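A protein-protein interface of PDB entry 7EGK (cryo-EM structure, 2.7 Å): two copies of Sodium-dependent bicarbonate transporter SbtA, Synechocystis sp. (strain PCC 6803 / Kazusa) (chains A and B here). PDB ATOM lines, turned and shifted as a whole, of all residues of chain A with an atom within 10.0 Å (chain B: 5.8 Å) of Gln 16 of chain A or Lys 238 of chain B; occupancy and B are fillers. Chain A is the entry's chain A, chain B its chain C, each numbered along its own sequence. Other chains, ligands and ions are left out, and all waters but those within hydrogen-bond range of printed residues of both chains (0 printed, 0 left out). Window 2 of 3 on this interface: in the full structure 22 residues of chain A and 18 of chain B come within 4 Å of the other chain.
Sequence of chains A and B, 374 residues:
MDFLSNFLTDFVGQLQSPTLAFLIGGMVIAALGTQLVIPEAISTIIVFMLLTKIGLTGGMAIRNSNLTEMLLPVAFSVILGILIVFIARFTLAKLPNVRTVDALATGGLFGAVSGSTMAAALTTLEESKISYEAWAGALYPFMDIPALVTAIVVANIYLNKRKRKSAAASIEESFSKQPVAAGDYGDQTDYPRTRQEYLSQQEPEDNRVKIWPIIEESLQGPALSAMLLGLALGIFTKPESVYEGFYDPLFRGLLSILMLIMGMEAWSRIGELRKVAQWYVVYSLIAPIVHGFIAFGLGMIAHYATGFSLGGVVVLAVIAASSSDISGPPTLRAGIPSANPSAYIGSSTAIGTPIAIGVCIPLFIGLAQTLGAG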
ATOM      1  N   LEU A   8     -27.344  17.405  -7.141  1.00  0.00           N
ATOM      2  CA  LEU A   8     -27.496  16.042  -6.636  1.00  0.00           C
ATOM      3  C   LEU A   8     -27.087  15.013  -7.685  1.00  0.00           C
ATOM      4  O   LEU A   8     -26.528  13.964  -7.345  1.00  0.00           O
ATOM      5  CB  LEU A   8     -28.931  15.815  -6.157  1.00  0.00           C
ATOM      6  CG  LEU A   8     -29.217  14.604  -5.259  1.00  0.00           C
ATOM      7  CD1 LEU A   8     -30.285  14.969  -4.244  1.00  0.00           C
ATOM      8  CD2 LEU A   8     -29.659  13.366  -6.033  1.00  0.00           C
ATOM      9  N   THR A   9     -27.350  15.292  -8.961  1.00  0.00           N
ATOM     10  CA  THR A   9     -26.859  14.404 -10.009  1.00  0.00           C
ATOM     11  C   THR A   9     -25.380  14.638 -10.299  1.00  0.00           C
ATOM     12  O   THR A   9     -24.737  13.809 -10.948  1.00  0.00           O
ATOM     13  CB  THR A   9     -27.686  14.572 -11.280  1.00  0.00           C
ATOM     14  OG1 THR A   9     -27.257  13.622 -12.264  1.00  0.00           O
ATOM     15  CG2 THR A   9     -27.552  15.983 -11.832  1.00  0.00           C
ATOM     16  N   ASP A  10     -24.824  15.756  -9.835  1.00  0.00           N
ATOM     17  CA  ASP A  10     -23.377  15.920  -9.845  1.00  0.00           C
ATOM     18  C   ASP A  10     -22.730  15.259  -8.640  1.00  0.00           C
ATOM     19  O   ASP A  10     -21.529  14.974  -8.668  1.00  0.00           O
ATOM     20  CB  ASP A  10     -23.004  17.405  -9.874  1.00  0.00           C
ATOM     21  CG  ASP A  10     -22.099  17.756 -11.038  1.00  0.00           C
ATOM     22  OD1 ASP A  10     -21.277  16.901 -11.430  1.00  0.00           O
ATOM     23  OD2 ASP A  10     -22.201  18.886 -11.558  1.00  0.00           O
ATOM     24  N   PHE A  11     -23.506  15.007  -7.589  1.00  0.00           N
ATOM     25  CA  PHE A  11     -22.954  14.371  -6.403  1.00  0.00           C
ATOM     26  C   PHE A  11     -22.808  12.871  -6.602  1.00  0.00           C
ATOM     27  O   PHE A  11     -21.777  12.292  -6.246  1.00  0.00           O
ATOM     28  CB  PHE A  11     -23.837  14.676  -5.200  1.00  0.00           C
ATOM     29  CG  PHE A  11     -23.312  14.134  -3.916  1.00  0.00           C
ATOM     30  CD1 PHE A  11     -23.983  13.121  -3.255  1.00  0.00           C
ATOM     31  CD2 PHE A  11     -22.143  14.628  -3.372  1.00  0.00           C
ATOM     32  CE1 PHE A  11     -23.505  12.620  -2.064  1.00  0.00           C
ATOM     33  CE2 PHE A  11     -21.656  14.130  -2.183  1.00  0.00           C
ATOM     34  CZ  PHE A  11     -22.336  13.123  -1.528  1.00  0.00           C
ATOM     35  N   VAL A  12     -23.819  12.226  -7.178  1.00  0.00           N
ATOM     36  CA  VAL A  12     -23.749  10.796  -7.446  1.00  0.00           C
ATOM     37  C   VAL A  12     -22.927  10.585  -8.715  1.00  0.00           C
ATOM     38  O   VAL A  12     -22.394   9.497  -8.949  1.00  0.00           O
ATOM     39  CB  VAL A  12     -25.160  10.177  -7.543  1.00  0.00           C
ATOM     40  CG1 VAL A  12     -25.893  10.629  -8.801  1.00  0.00           C
ATOM     41  CG2 VAL A  12     -25.118   8.651  -7.434  1.00  0.00           C
ATOM     42  N   GLY A  13     -22.794  11.629  -9.527  1.00  0.00           N
ATOM     43  CA  GLY A  13     -21.960  11.555 -10.709  1.00  0.00           C
ATOM     44  C   GLY A  13     -20.485  11.528 -10.368  1.00  0.00           C
ATOM     45  O   GLY A  13     -19.678  10.971 -11.117  1.00  0.00           O
ATOM     46  N   GLN A  14     -20.119  12.127  -9.232  1.00  0.00           N
ATOM     47  CA  GLN A  14     -18.733  12.072  -8.797  1.00  0.00           C
ATOM     48  C   GLN A  14     -18.443  10.876  -7.906  1.00  0.00           C
ATOM     49  O   GLN A  14     -17.286  10.456  -7.823  1.00  0.00           O
ATOM     50  CB  GLN A  14     -18.342  13.360  -8.082  1.00  0.00           C
ATOM     51  CG  GLN A  14     -16.916  13.769  -8.391  1.00  0.00           C
ATOM     52  CD  GLN A  14     -16.461  14.980  -7.615  1.00  0.00           C
ATOM     53  OE1 GLN A  14     -15.605  14.885  -6.737  1.00  0.00           O
ATOM     54  NE2 GLN A  14     -17.015  16.134  -7.951  1.00  0.00           N
ATOM     55  N   LEU A  15     -19.449  10.327  -7.236  1.00  0.00           N
ATOM     56  CA  LEU A  15     -19.273   9.053  -6.555  1.00  0.00           C
ATOM     57  C   LEU A  15     -19.152   7.888  -7.523  1.00  0.00           C
ATOM     58  O   LEU A  15     -18.596   6.854  -7.149  1.00  0.00           O
ATOM     59  CB  LEU A  15     -20.424   8.777  -5.584  1.00  0.00           C
ATOM     60  CG  LEU A  15     -20.272   9.361  -4.184  1.00  0.00           C
ATOM     61  CD1 LEU A  15     -21.505  10.138  -3.768  1.00  0.00           C
ATOM     62  CD2 LEU A  15     -19.948   8.257  -3.185  1.00  0.00           C
ATOM     63  N   GLN A  16     -19.639   8.031  -8.751  1.00  0.00           N
ATOM     64  CA  GLN A  16     -19.540   7.012  -9.786  1.00  0.00           C
ATOM     65  C   GLN A  16     -18.334   7.289 -10.666  1.00  0.00           C
ATOM     66  O   GLN A  16     -18.343   7.041 -11.873  1.00  0.00           O
ATOM     67  CB  GLN A  16     -20.815   6.954 -10.622  1.00  0.00           C
ATOM     68  CG  GLN A  16     -22.003   6.369  -9.900  1.00  0.00           C
ATOM     69  CD  GLN A  16     -21.968   4.869  -9.859  1.00  0.00           C
ATOM     70  OE1 GLN A  16     -21.750   4.218 -10.876  1.00  0.00           O
ATOM     71  NE2 GLN A  16     -22.174   4.306  -8.678  1.00  0.00           N
ATOM     72  N   SER A  17     -17.281   7.818 -10.064  1.00  0.00           N
ATOM     73  CA  SER A  17     -16.073   8.206 -10.775  1.00  0.00           C
ATOM     74  C   SER A  17     -14.905   7.991  -9.829  1.00  0.00           C
ATOM     75  O   SER A  17     -15.101   7.870  -8.615  1.00  0.00           O
ATOM     76  CB  SER A  17     -16.146   9.674 -11.226  1.00  0.00           C
ATOM     77  OG  SER A  17     -16.035  10.537 -10.111  1.00  0.00           O
ATOM     78  N   PRO A  18     -13.660   7.968 -10.345  1.00  0.00           N
ATOM     79  CA  PRO A  18     -12.515   8.005  -9.426  1.00  0.00           C
ATOM     80  C   PRO A  18     -12.371   9.362  -8.760  1.00  0.00           C
ATOM     81  O   PRO A  18     -13.218  10.244  -8.954  1.00  0.00           O
ATOM     82  CB  PRO A  18     -11.320   7.683 -10.330  1.00  0.00           C
ATOM     83  CG  PRO A  18     -11.778   8.001 -11.696  1.00  0.00           C
ATOM     84  CD  PRO A  18     -13.227   7.645 -11.715  1.00  0.00           C
ATOM     85  N   THR A  19     -11.338   9.504  -7.923  1.00  0.00           N
ATOM     86  CA  THR A  19     -10.911  10.681  -7.157  1.00  0.00           C
ATOM     87  C   THR A  19     -11.857  10.964  -5.980  1.00  0.00           C
ATOM     88  O   THR A  19     -11.497  11.715  -5.075  1.00  0.00           O
ATOM     89  CB  THR A  19     -10.751  11.932  -8.051  1.00  0.00           C
ATOM     90  OG1 THR A  19     -10.129  11.542  -9.280  1.00  0.00           O
ATOM     91  CG2 THR A  19      -9.833  12.955  -7.448  1.00  0.00           C
ATOM     92  N   LEU A  20     -13.015  10.316  -5.911  1.00  0.00           N
ATOM     93  CA  LEU A  20     -13.858  10.393  -4.730  1.00  0.00           C
ATOM     94  C   LEU A  20     -14.104   8.975  -4.249  1.00  0.00           C
ATOM     95  O   LEU A  20     -14.258   8.739  -3.050  1.00  0.00           O
ATOM     96  CB  LEU A  20     -15.179  11.099  -5.029  1.00  0.00           C
ATOM     97  CG  LEU A  20     -15.978  11.718  -3.878  1.00  0.00           C
ATOM     98  CD1 LEU A  20     -16.803  12.855  -4.428  1.00  0.00           C
ATOM     99  CD2 LEU A  20     -16.891  10.743  -3.158  1.00  0.00           C
ATOM    100  N   ALA A  21     -14.141   8.029  -5.186  1.00  0.00           N
ATOM    101  CA  ALA A  21     -14.325   6.635  -4.818  1.00  0.00           C
ATOM    102  C   ALA A  21     -13.115   6.080  -4.092  1.00  0.00           C
ATOM    103  O   ALA A  21     -13.264   5.254  -3.187  1.00  0.00           O
ATOM    104  CB  ALA A  21     -14.604   5.809  -6.058  1.00  0.00           C
ATOM    105  N   PHE A  22     -11.916   6.518  -4.467  1.00  0.00           N
ATOM    106  CA  PHE A  22     -10.731   6.098  -3.737  1.00  0.00           C
ATOM    107  C   PHE A  22     -10.641   6.786  -2.386  1.00  0.00           C
ATOM    108  O   PHE A  22     -10.006   6.262  -1.471  1.00  0.00           O
ATOM    109  CB  PHE A  22      -9.485   6.375  -4.567  1.00  0.00           C
ATOM    110  CG  PHE A  22      -9.221   5.349  -5.622  1.00  0.00           C
ATOM    111  CD1 PHE A  22      -9.834   5.436  -6.854  1.00  0.00           C
ATOM    112  CD2 PHE A  22      -8.350   4.304  -5.385  1.00  0.00           C
ATOM    113  CE1 PHE A  22      -9.588   4.496  -7.832  1.00  0.00           C
ATOM    114  CE2 PHE A  22      -8.100   3.362  -6.359  1.00  0.00           C
ATOM    115  CZ  PHE A  22      -8.720   3.460  -7.583  1.00  0.00           C
ATOM    116  N   ILE A  24     -13.490   7.398  -0.575  1.00  0.00           N
ATOM    117  CA  ILE A  24     -14.430   6.577   0.180  1.00  0.00           C
ATOM    118  C   ILE A  24     -13.875   5.175   0.376  1.00  0.00           C
ATOM    119  O   ILE A  24     -14.029   4.586   1.452  1.00  0.00           O
ATOM    120  CB  ILE A  24     -15.801   6.557  -0.525  1.00  0.00           C
ATOM    121  CG1 ILE A  24     -16.362   7.968  -0.650  1.00  0.00           C
ATOM    122  CG2 ILE A  24     -16.802   5.707   0.222  1.00  0.00           C
ATOM    123  CD1 ILE A  24     -16.466   8.694   0.656  1.00  0.00           C
ATOM    124  N   GLU A 127     -12.301  16.533 -16.720  1.00  0.00           N
ATOM    125  CA  GLU A 127     -13.288  15.596 -17.238  1.00  0.00           C
ATOM    126  C   GLU A 127     -14.718  16.103 -17.115  1.00  0.00           C
ATOM    127  O   GLU A 127     -15.645  15.379 -17.487  1.00  0.00           O
ATOM    128  CB  GLU A 127     -13.153  14.231 -16.563  1.00  0.00           C
ATOM    129  CG  GLU A 127     -11.726  13.788 -16.287  1.00  0.00           C
ATOM    130  CD  GLU A 127     -11.569  13.107 -14.944  1.00  0.00           C
ATOM    131  OE1 GLU A 127     -12.600  12.782 -14.323  1.00  0.00           O
ATOM    132  OE2 GLU A 127     -10.416  12.874 -14.523  1.00  0.00           O
ATOM    133  N   GLY A 358     -15.644  15.653  -1.184  1.00  0.00           N
ATOM    134  CA  GLY A 358     -16.919  15.019  -1.422  1.00  0.00           C
ATOM    135  C   GLY A 358     -18.059  15.961  -1.738  1.00  0.00           C
ATOM    136  O   GLY A 358     -18.857  15.683  -2.632  1.00  0.00           O
ATOM    137  N   PRO A 362     -18.154  18.917  -6.132  1.00  0.00           N
ATOM    138  CA  PRO A 362     -19.306  18.911  -7.048  1.00  0.00           C
ATOM    139  C   PRO A 362     -20.304  20.027  -6.803  1.00  0.00           C
ATOM    140  O   PRO A 362     -21.219  20.196  -7.615  1.00  0.00           O
ATOM    141  CB  PRO A 362     -19.941  17.543  -6.805  1.00  0.00           C
ATOM    142  CG  PRO A 362     -19.630  17.256  -5.442  1.00  0.00           C
ATOM    143  CD  PRO A 362     -18.245  17.742  -5.238  1.00  0.00           C
ATOM    144  N   ARG B  63     -20.519  -6.941 -12.555  1.00  0.00           N
ATOM    145  CA  ARG B  63     -21.766  -6.202 -12.700  1.00  0.00           C
ATOM    146  C   ARG B  63     -22.449  -6.451 -14.039  1.00  0.00           C
ATOM    147  O   ARG B  63     -23.637  -6.143 -14.178  1.00  0.00           O
ATOM    148  CB  ARG B  63     -21.517  -4.706 -12.508  1.00  0.00           C
ATOM    149  CG  ARG B  63     -20.592  -4.080 -13.526  1.00  0.00           C
ATOM    150  CD  ARG B  63     -20.692  -2.567 -13.472  1.00  0.00           C
ATOM    151  NE  ARG B  63     -19.917  -1.923 -14.527  1.00  0.00           N
ATOM    152  CZ  ARG B  63     -18.931  -1.062 -14.308  1.00  0.00           C
ATOM    153  NH1 ARG B  63     -18.596  -0.737 -13.070  1.00  0.00           N
ATOM    154  NH2 ARG B  63     -18.280  -0.522 -15.326  1.00  0.00           N
ATOM    155  N   LEU B 233     -14.659  -1.197  -6.234  1.00  0.00           N
ATOM    156  CA  LEU B 233     -14.628  -0.042  -7.121  1.00  0.00           C
ATOM    157  C   LEU B 233     -14.988  -0.433  -8.546  1.00  0.00           C
ATOM    158  O   LEU B 233     -15.414   0.410  -9.337  1.00  0.00           O
ATOM    159  CB  LEU B 233     -13.257   0.624  -7.078  1.00  0.00           C
ATOM    160  CG  LEU B 233     -12.877   1.267  -5.746  1.00  0.00           C
ATOM    161  CD1 LEU B 233     -11.545   1.957  -5.851  1.00  0.00           C
ATOM    162  CD2 LEU B 233     -13.934   2.231  -5.289  1.00  0.00           C
ATOM    163  N   GLY B 234     -14.823  -1.704  -8.896  1.00  0.00           N
ATOM    164  CA  GLY B 234     -15.256  -2.145 -10.208  1.00  0.00           C
ATOM    165  C   GLY B 234     -16.762  -2.285 -10.304  1.00  0.00           C
ATOM    166  O   GLY B 234     -17.355  -1.981 -11.339  1.00  0.00           O
ATOM    167  N   PHE B 236     -19.404  -0.997  -8.063  1.00  0.00           N
ATOM    168  CA  PHE B 236     -20.277   0.108  -7.697  1.00  0.00           C
ATOM    169  C   PHE B 236     -19.907   1.430  -8.353  1.00  0.00           C
ATOM    170  O   PHE B 236     -20.678   2.388  -8.250  1.00  0.00           O
ATOM    171  CB  PHE B 236     -20.281   0.287  -6.177  1.00  0.00           C
ATOM    172  CG  PHE B 236     -20.711  -0.936  -5.427  1.00  0.00           C
ATOM    173  CD1 PHE B 236     -21.992  -1.434  -5.572  1.00  0.00           C
ATOM    174  CD2 PHE B 236     -19.835  -1.587  -4.577  1.00  0.00           C
ATOM    175  CE1 PHE B 236     -22.392  -2.559  -4.883  1.00  0.00           C
ATOM    176  CE2 PHE B 236     -20.227  -2.714  -3.888  1.00  0.00           C
ATOM    177  CZ  PHE B 236     -21.507  -3.199  -4.041  1.00  0.00           C
ATOM    178  N   THR B 237     -18.763   1.514  -9.016  1.00  0.00           N
ATOM    179  CA  THR B 237     -18.230   2.772  -9.518  1.00  0.00           C
ATOM    180  C   THR B 237     -17.879   2.568 -11.001  1.00  0.00           C
ATOM    181  O   THR B 237     -18.086   1.491 -11.555  1.00  0.00           O
ATOM    182  CB  THR B 237     -17.048   3.189  -8.629  1.00  0.00           C
ATOM    183  OG1 THR B 237     -17.391   2.944  -7.263  1.00  0.00           O
ATOM    184  CG2 THR B 237     -16.771   4.668  -8.708  1.00  0.00           C
ATOM    185  N   LYS B 238     -17.376   3.616 -11.655  1.00  0.00           N
ATOM    186  CA  LYS B 238     -16.924   3.560 -13.044  1.00  0.00           C
ATOM    187  C   LYS B 238     -15.458   3.973 -13.098  1.00  0.00           C
ATOM    188  O   LYS B 238     -15.136   5.131 -13.394  1.00  0.00           O
ATOM    189  CB  LYS B 238     -17.797   4.450 -13.926  1.00  0.00           C
ATOM    190  CG  LYS B 238     -19.212   3.937 -14.040  1.00  0.00           C
ATOM    191  CD  LYS B 238     -20.126   4.949 -14.683  1.00  0.00           C
ATOM    192  CE  LYS B 238     -21.555   4.445 -14.698  1.00  0.00           C
ATOM    193  NZ  LYS B 238     -22.503   5.502 -15.134  1.00  0.00           N
ATOM    194  N   PRO B 239     -14.538   3.047 -12.809  1.00  0.00           N
ATOM    195  CA  PRO B 239     -13.115   3.396 -12.745  1.00  0.00           C
ATOM    196  C   PRO B 239     -12.360   3.246 -14.057  1.00  0.00           C
ATOM    197  O   PRO B 239     -11.133   3.131 -14.032  1.00  0.00           O
ATOM    198  CB  PRO B 239     -12.585   2.419 -11.695  1.00  0.00           C
ATOM    199  CG  PRO B 239     -13.399   1.210 -11.918  1.00  0.00           C
ATOM    200  CD  PRO B 239     -14.756   1.647 -12.418  1.00  0.00           C
ATOM    201  N   GLU B 240     -13.070   3.214 -15.192  1.00  0.00           N
ATOM    202  CA  GLU B 240     -12.462   2.888 -16.483  1.00  0.00           C
ATOM    203  C   GLU B 240     -11.409   3.899 -16.923  1.00  0.00           C
ATOM    204  O   GLU B 240     -10.517   3.555 -17.703  1.00  0.00           O
ATOM    205  CB  GLU B 240     -13.539   2.798 -17.561  1.00  0.00           C
ATOM    206  CG  GLU B 240     -14.462   1.613 -17.444  1.00  0.00           C
ATOM    207  CD  GLU B 240     -15.732   1.940 -16.694  1.00  0.00           C
ATOM    208  OE1 GLU B 240     -16.592   1.048 -16.555  1.00  0.00           O
ATOM    209  OE2 GLU B 240     -15.870   3.092 -16.243  1.00  0.00           O
ATOM    210  N   SER B 241     -11.496   5.142 -16.455  1.00  0.00           N
ATOM    211  CA  SER B 241     -10.543   6.155 -16.892  1.00  0.00           C
ATOM    212  C   SER B 241      -9.190   5.975 -16.213  1.00  0.00           C
ATOM    213  O   SER B 241      -8.144   6.090 -16.859  1.00  0.00           O
ATOM    214  CB  SER B 241     -11.104   7.549 -16.629  1.00  0.00           C
ATOM    215  OG  SER B 241     -11.120   7.841 -15.245  1.00  0.00           O
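O of Phe 236 of chain B lies within hydrogen-bond range of NE2 of Gln 16 of chain A (2.5 Å).
The backbone carbonyl oxygen (O) of Thr 237 of chain B sits at hydrogen-bond distance from the guanidinium group (NH1) of Arg 63 of chain B (2.7 Å). OG of Ser 17 of chain A sits at hydrogen-bond distance from O of Gln 14 of chain A (2.6 Å).
O of Leu 15 of chain A touches CG2 of Thr 237 of chain B (3.2 Å). Gln 16 of chain A touches Thr 237 of chain B (C to CG2, 3.6 Å). Lys 238 of chain B touches Gln 16 of chain A (CB to O, 3.4 Å). Ser 17 of chain A touches Thr 237 of chain B (N to CG2, 3.5 Å). Pro 18 of chain A touches Lys 238 of chain B. OG of Ser 241 of chain B touches CG of Pro 18 of chain A, 3.6 Å away. CD2 of Leu 233 of chain B touches CB of Ala 21 of chain A (3.7 Å). CG2 of Thr 237 of chain B touches CB of Ala 21 of chain A, at 3.6 Å. CZ of Phe 22 of chain A touches CD1 of Leu 233 of chain B, 3.6 Å away.
Gln 16 of chain A touches just these residues of chain B: Phe 236, Thr 237 and Lys 238. Of the printed residues of chain A, Lys 238 of chain B touches Gln 16 and Pro 18. Of chain A, only Leu 15, Gln 16, Ser 17 and Ala 21 come within 4 Å of Thr 237 of chain B. No residue of chain A comes within 4 Å of Pro 239 of chain B. Of the printed residues of chain B, Leu 15 of chain A touches Thr 237 (3.2 Å). Printed residues of chain B within 4 Å of Pro 18 of chain A: Lys 238 and Ser 241. Printed residues of chain A within 4 Å of Ser 241 of chain B: Pro 18. Printed residues of chain A within 4 Å of Phe 236 of chain B: Gln 16 (2.5 Å). The nearest residue of chain A that does not touch Lys 238 of chain B is Ser 17 of chain A (4.1 Å). The nearest printed residue of chain B that does not touch Leu 15 of chain A is Phe 236 of chain B (5.0 Å).
Of the 9 printed residues of chain B, 5 touch a printed residue of chain A. Printed residues of chain B that touch a printed residue of chain A: Leu 233, Phe 236, Thr 237, Lys 238 and Ser 241. Hydrophobic or aromatic side chains of chain B within 4 Å of the printed part of chain A: Leu 233. Of the 19 printed residues of chain A, 6 touch a printed residue of chain B. Hydrophobic or aromatic side chains of chain A that line the printed part of chain B: Pro 18, Ala 21 and Phe 22. Among the printed residues, no Asp or Glu carboxylate lies within 4 Å of a Lys or Arg side-chain nitrogen of the other chain.
No position is printed for both chains. Of the 10 pairs that touch across the chains among the printed residues, none has its exchanged pair printed and touching as well.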
